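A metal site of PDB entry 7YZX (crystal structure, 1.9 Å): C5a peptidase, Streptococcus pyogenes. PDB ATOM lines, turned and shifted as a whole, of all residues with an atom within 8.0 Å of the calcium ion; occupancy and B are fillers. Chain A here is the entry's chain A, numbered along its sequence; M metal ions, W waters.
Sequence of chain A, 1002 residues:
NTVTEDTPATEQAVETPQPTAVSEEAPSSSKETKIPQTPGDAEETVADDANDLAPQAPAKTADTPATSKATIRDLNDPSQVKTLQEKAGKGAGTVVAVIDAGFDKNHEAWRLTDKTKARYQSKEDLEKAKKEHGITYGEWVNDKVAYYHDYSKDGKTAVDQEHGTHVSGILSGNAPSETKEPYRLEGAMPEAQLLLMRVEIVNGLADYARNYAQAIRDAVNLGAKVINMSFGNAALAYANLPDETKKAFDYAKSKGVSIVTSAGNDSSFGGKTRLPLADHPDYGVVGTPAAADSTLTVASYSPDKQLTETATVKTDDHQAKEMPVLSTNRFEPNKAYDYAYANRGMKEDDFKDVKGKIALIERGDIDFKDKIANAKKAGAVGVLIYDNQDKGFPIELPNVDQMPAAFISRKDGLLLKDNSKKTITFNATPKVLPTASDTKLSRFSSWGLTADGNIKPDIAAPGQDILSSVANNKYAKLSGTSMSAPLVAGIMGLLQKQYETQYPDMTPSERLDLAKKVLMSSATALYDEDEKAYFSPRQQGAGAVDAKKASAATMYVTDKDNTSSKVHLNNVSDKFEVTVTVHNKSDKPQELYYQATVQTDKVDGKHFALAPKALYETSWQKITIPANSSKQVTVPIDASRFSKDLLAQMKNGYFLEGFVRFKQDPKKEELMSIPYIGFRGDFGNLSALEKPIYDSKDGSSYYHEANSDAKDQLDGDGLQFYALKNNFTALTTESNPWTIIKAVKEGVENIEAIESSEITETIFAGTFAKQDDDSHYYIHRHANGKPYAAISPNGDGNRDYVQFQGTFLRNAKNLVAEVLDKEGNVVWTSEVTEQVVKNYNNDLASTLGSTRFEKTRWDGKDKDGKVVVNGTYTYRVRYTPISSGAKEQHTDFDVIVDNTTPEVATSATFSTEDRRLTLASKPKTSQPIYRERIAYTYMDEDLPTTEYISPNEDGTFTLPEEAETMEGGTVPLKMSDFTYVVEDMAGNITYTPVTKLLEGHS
Five residues have an atom within 4 Å of the calcium ion: Ser 792, Asn 794, Asp 796, Asn 798 and Asp 800.
Water W1 lies within hydrogen-bond range of the backbone carbonyl oxygen (O) of Gly 987 (2.7 Å), the side-chain carboxylate (OD2) of Asp 796 (2.7 Å) and the side-chain amide nitrogen (ND2) of Asn 794 (3.1 Å).
The backbone NH (N) of Gly 797 lies within hydrogen-bond range of the side-chain carboxylate (OD2) of Asp 800 (2.6 Å).
The backbone carbonyl oxygen (O) of Gly 987 is in hydrogen-bond range of the side-chain amide nitrogen (ND2) of Asn 798 (3.0 Å).
The backbone NH (N) of Asn 736 is in hydrogen-bond range of the side-chain amide oxygen (OD1) of Asn 798 (3.0 Å).
The side-chain amide nitrogen (ND2) of Asn 798 is in hydrogen-bond range of the side-chain carboxylate (OE2) of Glu 983 (2.8 Å).
The backbone carbonyl oxygen of Asp 796 is in hydrogen-bond range of the side-chain amide nitrogen of Asn 736.
O of Arg 799 lies within hydrogen-bond range of N of Ser 792 (2.9 Å).
O of Ala 986 lies close to N of Ser 792 (3.3 Å).
The side-chain amide nitrogen (ND2) of Asn 794 sits at hydrogen-bond distance from the side-chain amide oxygen (OD1) of Asn 988 (3.5 Å).
The side-chain carboxylate (OD1) of Asp 800 binds the calcium ion, 2.3 Å away.
The calcium ion is bound by water W1 (2.4 Å).
O of Asn 798 binds the calcium ion (2.5 Å).
The side-chain carboxylate (OD1) of Asp 796 is bound to the calcium ion, at 2.5 Å.
The calcium ion is bound by O of Ser 792.
The side-chain amide oxygen (OD1) of Asn 794 is bound to the calcium ion (2.5 Å).
The side-chain hydroxyl (OG) of Ser 792 binds the calcium ion (2.6 Å).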
ATOM      1  N   GLU A 734     -33.938   1.398   2.392  1.00  0.00           N
ATOM      2  CA  GLU A 734     -34.434   2.751   2.155  1.00  0.00           C
ATOM      3  C   GLU A 734     -33.479   3.510   1.247  1.00  0.00           C
ATOM      4  O   GLU A 734     -32.258   3.341   1.315  1.00  0.00           O
ATOM      5  CB  GLU A 734     -34.660   3.521   3.458  1.00  0.00           C
ATOM      6  CG  GLU A 734     -35.958   3.134   4.147  1.00  0.00           C
ATOM      7  CD  GLU A 734     -36.241   3.945   5.400  1.00  0.00           C
ATOM      8  OE1 GLU A 734     -36.162   5.191   5.339  1.00  0.00           O
ATOM      9  OE2 GLU A 734     -36.551   3.332   6.441  1.00  0.00           O
ATOM     10  N   ASN A 736     -32.364   7.371   0.246  1.00  0.00           N
ATOM     11  CA  ASN A 736     -32.362   8.713   0.815  1.00  0.00           C
ATOM     12  C   ASN A 736     -31.582   9.639  -0.113  1.00  0.00           C
ATOM     13  O   ASN A 736     -30.363   9.466  -0.274  1.00  0.00           O
ATOM     14  CB  ASN A 736     -31.762   8.704   2.213  1.00  0.00           C
ATOM     15  CG  ASN A 736     -32.285   9.826   3.078  1.00  0.00           C
ATOM     16  OD1 ASN A 736     -33.330  10.420   2.774  1.00  0.00           O
ATOM     17  ND2 ASN A 736     -31.581  10.131   4.167  1.00  0.00           N
ATOM     18  N   ILE A 741     -29.946  14.107   2.910  1.00  0.00           N
ATOM     19  CA  ILE A 741     -28.757  13.814   3.703  1.00  0.00           C
ATOM     20  C   ILE A 741     -28.063  15.103   4.127  1.00  0.00           C
ATOM     21  O   ILE A 741     -27.567  15.222   5.251  1.00  0.00           O
ATOM     22  CB  ILE A 741     -27.804  12.905   2.908  1.00  0.00           C
ATOM     23  CG1 ILE A 741     -28.484  11.585   2.544  1.00  0.00           C
ATOM     24  CG2 ILE A 741     -26.531  12.638   3.701  1.00  0.00           C
ATOM     25  CD1 ILE A 741     -27.600  10.619   1.775  1.00  0.00           C
ATOM     26  N   ALA A 790     -26.727  -4.627  -1.144  1.00  0.00           N
ATOM     27  CA  ALA A 790     -25.561  -3.986  -0.544  1.00  0.00           C
ATOM     28  C   ALA A 790     -25.998  -2.852   0.373  1.00  0.00           C
ATOM     29  O   ALA A 790     -26.927  -2.108   0.051  1.00  0.00           O
ATOM     30  CB  ALA A 790     -24.605  -3.453  -1.617  1.00  0.00           C
ATOM     31  N   ILE A 791     -25.318  -2.725   1.516  1.00  0.00           N
ATOM     32  CA  ILE A 791     -25.616  -1.671   2.472  1.00  0.00           C
ATOM     33  C   ILE A 791     -24.342  -0.907   2.808  1.00  0.00           C
ATOM     34  O   ILE A 791     -23.232  -1.434   2.718  1.00  0.00           O
ATOM     35  CB  ILE A 791     -26.268  -2.220   3.755  1.00  0.00           C
ATOM     36  CG1 ILE A 791     -25.439  -3.355   4.348  1.00  0.00           C
ATOM     37  CG2 ILE A 791     -27.698  -2.662   3.487  1.00  0.00           C
ATOM     38  CD1 ILE A 791     -25.897  -3.783   5.725  1.00  0.00           C
ATOM     39  N   SER A 792     -24.526   0.342   3.205  1.00  0.00           N
ATOM     40  CA  SER A 792     -23.436   1.228   3.639  1.00  0.00           C
ATOM     41  C   SER A 792     -23.845   1.778   4.994  1.00  0.00           C
ATOM     42  O   SER A 792     -24.440   2.856   5.088  1.00  0.00           O
ATOM     43  CB  SER A 792     -23.191   2.346   2.632  1.00  0.00           C
ATOM     44  OG  SER A 792     -24.380   3.064   2.383  1.00  0.00           O
ATOM     45  N   PRO A 793     -23.559   1.053   6.072  1.00  0.00           N
ATOM     46  CA  PRO A 793     -24.030   1.458   7.423  1.00  0.00           C
ATOM     47  C   PRO A 793     -23.237   2.630   8.006  1.00  0.00           C
ATOM     48  O   PRO A 793     -22.393   2.495   8.874  1.00  0.00           O
ATOM     49  CB  PRO A 793     -23.858   0.177   8.238  1.00  0.00           C
ATOM     50  CG  PRO A 793     -22.725  -0.533   7.583  1.00  0.00           C
ATOM     51  CD  PRO A 793     -22.828  -0.225   6.109  1.00  0.00           C
ATOM     52  N   ASN A 794     -23.549   3.828   7.510  1.00  0.00           N
ATOM     53  CA  ASN A 794     -22.902   5.057   7.980  1.00  0.00           C
ATOM     54  C   ASN A 794     -23.918   6.064   8.514  1.00  0.00           C
ATOM     55  O   ASN A 794     -23.632   7.267   8.549  1.00  0.00           O
ATOM     56  CB  ASN A 794     -22.059   5.673   6.856  1.00  0.00           C
ATOM     57  CG  ASN A 794     -22.805   5.771   5.541  1.00  0.00           C
ATOM     58  OD1 ASN A 794     -24.034   5.701   5.512  1.00  0.00           O
ATOM     59  ND2 ASN A 794     -22.070   5.952   4.459  1.00  0.00           N
ATOM     60  N   GLY A 795     -25.100   5.599   8.897  1.00  0.00           N
ATOM     61  CA  GLY A 795     -26.064   6.428   9.598  1.00  0.00           C
ATOM     62  C   GLY A 795     -26.713   7.534   8.800  1.00  0.00           C
ATOM     63  O   GLY A 795     -27.375   8.394   9.400  1.00  0.00           O
ATOM     64  N   ASP A 796     -26.578   7.561   7.479  1.00  0.00           N
ATOM     65  CA  ASP A 796     -27.164   8.650   6.697  1.00  0.00           C
ATOM     66  C   ASP A 796     -28.549   8.315   6.131  1.00  0.00           C
ATOM     67  O   ASP A 796     -29.177   9.186   5.542  1.00  0.00           O
ATOM     68  CB  ASP A 796     -26.225   9.080   5.563  1.00  0.00           C
ATOM     69  CG  ASP A 796     -26.061   8.016   4.488  1.00  0.00           C
ATOM     70  OD1 ASP A 796     -26.581   6.887   4.636  1.00  0.00           O
ATOM     71  OD2 ASP A 796     -25.391   8.311   3.475  1.00  0.00           O
ATOM     72  N   GLY A 797     -29.020   7.085   6.319  1.00  0.00           N
ATOM     73  CA  GLY A 797     -30.344   6.714   5.867  1.00  0.00           C
ATOM     74  C   GLY A 797     -30.431   6.224   4.428  1.00  0.00           C
ATOM     75  O   GLY A 797     -31.527   5.870   3.981  1.00  0.00           O
ATOM     76  N   ASN A 798     -29.316   6.195   3.700  1.00  0.00           N
ATOM     77  CA  ASN A 798     -29.314   5.724   2.318  1.00  0.00           C
ATOM     78  C   ASN A 798     -28.753   4.308   2.298  1.00  0.00           C
ATOM     79  O   ASN A 798     -27.535   4.117   2.414  1.00  0.00           O
ATOM     80  CB  ASN A 798     -28.505   6.655   1.429  1.00  0.00           C
ATOM     81  CG  ASN A 798     -28.701   6.352  -0.041  1.00  0.00           C
ATOM     82  OD1 ASN A 798     -29.796   5.982  -0.472  1.00  0.00           O
ATOM     83  ND2 ASN A 798     -27.635   6.489  -0.833  1.00  0.00           N
ATOM     84  N   ARG A 799     -29.639   3.326   2.136  1.00  0.00           N
ATOM     85  CA  ARG A 799     -29.241   1.913   2.027  1.00  0.00           C
ATOM     86  C   ARG A 799     -28.405   1.489   3.233  1.00  0.00           C
ATOM     87  O   ARG A 799     -27.339   0.873   3.090  1.00  0.00           O
ATOM     88  CB  ARG A 799     -28.512   1.645   0.708  1.00  0.00           C
ATOM     89  CG  ARG A 799     -29.410   1.840  -0.510  1.00  0.00           C
ATOM     90  CD  ARG A 799     -28.656   1.966  -1.816  1.00  0.00           C
ATOM     91  NE  ARG A 799     -29.551   2.328  -2.911  1.00  0.00           N
ATOM     92  CZ  ARG A 799     -30.168   1.450  -3.701  1.00  0.00           C
ATOM     93  NH1 ARG A 799     -29.985   0.149  -3.526  1.00  0.00           N
ATOM     94  NH2 ARG A 799     -30.978   1.873  -4.657  1.00  0.00           N
ATOM     95  N   ASP A 800     -28.894   1.822   4.431  1.00  0.00           N
ATOM     96  CA  ASP A 800     -28.201   1.509   5.673  1.00  0.00           C
ATOM     97  C   ASP A 800     -28.478   0.104   6.182  1.00  0.00           C
ATOM     98  O   ASP A 800     -27.676  -0.427   6.947  1.00  0.00           O
ATOM     99  CB  ASP A 800     -28.587   2.513   6.771  1.00  0.00           C
ATOM    100  CG  ASP A 800     -27.992   3.886   6.552  1.00  0.00           C
ATOM    101  OD1 ASP A 800     -27.201   4.059   5.608  1.00  0.00           O
ATOM    102  OD2 ASP A 800     -28.321   4.802   7.339  1.00  0.00           O
ATOM    103  N   TYR A 801     -29.591  -0.500   5.778  1.00  0.00           N
ATOM    104  CA  TYR A 801     -30.040  -1.734   6.403  1.00  0.00           C
ATOM    105  C   TYR A 801     -30.765  -2.607   5.381  1.00  0.00           C
ATOM    106  O   TYR A 801     -31.137  -2.155   4.293  1.00  0.00           O
ATOM    107  CB  TYR A 801     -30.967  -1.446   7.592  1.00  0.00           C
ATOM    108  CG  TYR A 801     -32.314  -0.849   7.217  1.00  0.00           C
ATOM    109  CD1 TYR A 801     -33.376  -1.667   6.841  1.00  0.00           C
ATOM    110  CD2 TYR A 801     -32.530   0.522   7.245  1.00  0.00           C
ATOM    111  CE1 TYR A 801     -34.603  -1.145   6.499  1.00  0.00           C
ATOM    112  CE2 TYR A 801     -33.760   1.057   6.908  1.00  0.00           C
ATOM    113  CZ  TYR A 801     -34.791   0.214   6.533  1.00  0.00           C
ATOM    114  OH  TYR A 801     -36.026   0.726   6.193  1.00  0.00           O
ATOM    115  N   ASP A 898     -20.236  -2.332   2.631  1.00  0.00           N
ATOM    116  CA  ASP A 898     -19.153  -1.505   2.122  1.00  0.00           C
ATOM    117  C   ASP A 898     -19.403  -0.063   2.569  1.00  0.00           C
ATOM    118  O   ASP A 898     -20.408   0.533   2.187  1.00  0.00           O
ATOM    119  CB  ASP A 898     -19.060  -1.598   0.602  1.00  0.00           C
ATOM    120  CG  ASP A 898     -17.730  -1.088   0.063  1.00  0.00           C
ATOM    121  OD1 ASP A 898     -17.295   0.013   0.464  1.00  0.00           O
ATOM    122  OD2 ASP A 898     -17.110  -1.790  -0.760  1.00  0.00           O
ATOM    123  N   ASN A 899     -18.475   0.483   3.359  1.00  0.00           N
ATOM    124  CA  ASN A 899     -18.584   1.845   3.880  1.00  0.00           C
ATOM    125  C   ASN A 899     -17.621   2.813   3.204  1.00  0.00           C
ATOM    126  O   ASN A 899     -17.494   3.956   3.659  1.00  0.00           O
ATOM    127  CB  ASN A 899     -18.346   1.843   5.388  1.00  0.00           C
ATOM    128  CG  ASN A 899     -19.634   1.730   6.175  1.00  0.00           C
ATOM    129  OD1 ASN A 899     -19.765   0.859   7.034  1.00  0.00           O
ATOM    130  ND2 ASN A 899     -20.579   2.617   5.897  1.00  0.00           N
ATOM    131  N   GLU A 983     -22.490   8.300  -6.461  1.00  0.00           N
ATOM    132  CA  GLU A 983     -23.056   7.275  -5.595  1.00  0.00           C
ATOM    133  C   GLU A 983     -22.658   5.893  -6.106  1.00  0.00           C
ATOM    134  O   GLU A 983     -22.676   5.657  -7.314  1.00  0.00           O
ATOM    135  CB  GLU A 983     -24.577   7.400  -5.532  1.00  0.00           C
ATOM    136  CG  GLU A 983     -25.275   6.449  -4.560  1.00  0.00           C
ATOM    137  CD  GLU A 983     -26.777   6.665  -4.515  1.00  0.00           C
ATOM    138  OE1 GLU A 983     -27.300   7.411  -5.379  1.00  0.00           O
ATOM    139  OE2 GLU A 983     -27.437   6.106  -3.611  1.00  0.00           O
ATOM    140  N   ASP A 984     -22.286   5.002  -5.199  1.00  0.00           N
ATOM    141  CA  ASP A 984     -21.966   3.633  -5.580  1.00  0.00           C
ATOM    142  C   ASP A 984     -23.145   2.714  -5.253  1.00  0.00           C
ATOM    143  O   ASP A 984     -24.162   3.133  -4.702  1.00  0.00           O
ATOM    144  CB  ASP A 984     -20.654   3.156  -4.916  1.00  0.00           C
ATOM    145  CG  ASP A 984     -20.769   2.926  -3.406  1.00  0.00           C
ATOM    146  OD1 ASP A 984     -21.881   2.959  -2.831  1.00  0.00           O
ATOM    147  OD2 ASP A 984     -19.715   2.704  -2.773  1.00  0.00           O
ATOM    148  N   ALA A 986     -23.606   0.501  -3.130  1.00  0.00           N
ATOM    149  CA  ALA A 986     -23.893   0.277  -1.722  1.00  0.00           C
ATOM    150  C   ALA A 986     -24.550   1.488  -1.057  1.00  0.00           C
ATOM    151  O   ALA A 986     -24.919   1.403   0.115  1.00  0.00           O
ATOM    152  CB  ALA A 986     -22.618  -0.101  -0.962  1.00  0.00           C
ATOM    153  N   GLY A 987     -24.692   2.595  -1.783  1.00  0.00           N
ATOM    154  CA  GLY A 987     -25.287   3.786  -1.223  1.00  0.00           C
ATOM    155  C   GLY A 987     -24.303   4.813  -0.698  1.00  0.00           C
ATOM    156  O   GLY A 987     -24.745   5.877  -0.239  1.00  0.00           O
ATOM    157  N   ASN A 988     -23.005   4.531  -0.729  1.00  0.00           N
ATOM    158  CA  ASN A 988     -22.012   5.536  -0.368  1.00  0.00           C
ATOM    159  C   ASN A 988     -22.066   6.675  -1.377  1.00  0.00           C
ATOM    160  O   ASN A 988     -22.068   6.444  -2.588  1.00  0.00           O
ATOM    161  CB  ASN A 988     -20.612   4.927  -0.337  1.00  0.00           C
ATOM    162  CG  ASN A 988     -20.475   3.846   0.724  1.00  0.00           C
ATOM    163  OD1 ASN A 988     -20.521   4.129   1.918  1.00  0.00           O
ATOM    164  ND2 ASN A 988     -20.296   2.607   0.283  1.00  0.00           N
ATOM    165  N   ILE A 989     -22.094   7.914  -0.875  1.00  0.00           N
ATOM    166  CA  ILE A 989     -22.442   9.065  -1.697  1.00  0.00           C
ATOM    167  C   ILE A 989     -21.610  10.272  -1.284  1.00  0.00           C
ATOM    168  O   ILE A 989     -21.355  10.487  -0.088  1.00  0.00           O
ATOM    169  CB  ILE A 989     -23.954   9.366  -1.599  1.00  0.00           C
ATOM    170  CG1 ILE A 989     -24.375  10.473  -2.557  1.00  0.00           C
ATOM    171  CG2 ILE A 989     -24.344   9.695  -0.160  1.00  0.00           C
ATOM    172  CD1 ILE A 989     -25.862  10.708  -2.567  1.00  0.00           C
HETATM  173 CA    CA M   1     -25.698   4.677   3.961  1.00  0.00          CA
HETATM  174  O   HOH W   1     -24.436   6.032   2.397  1.00  0.00           O
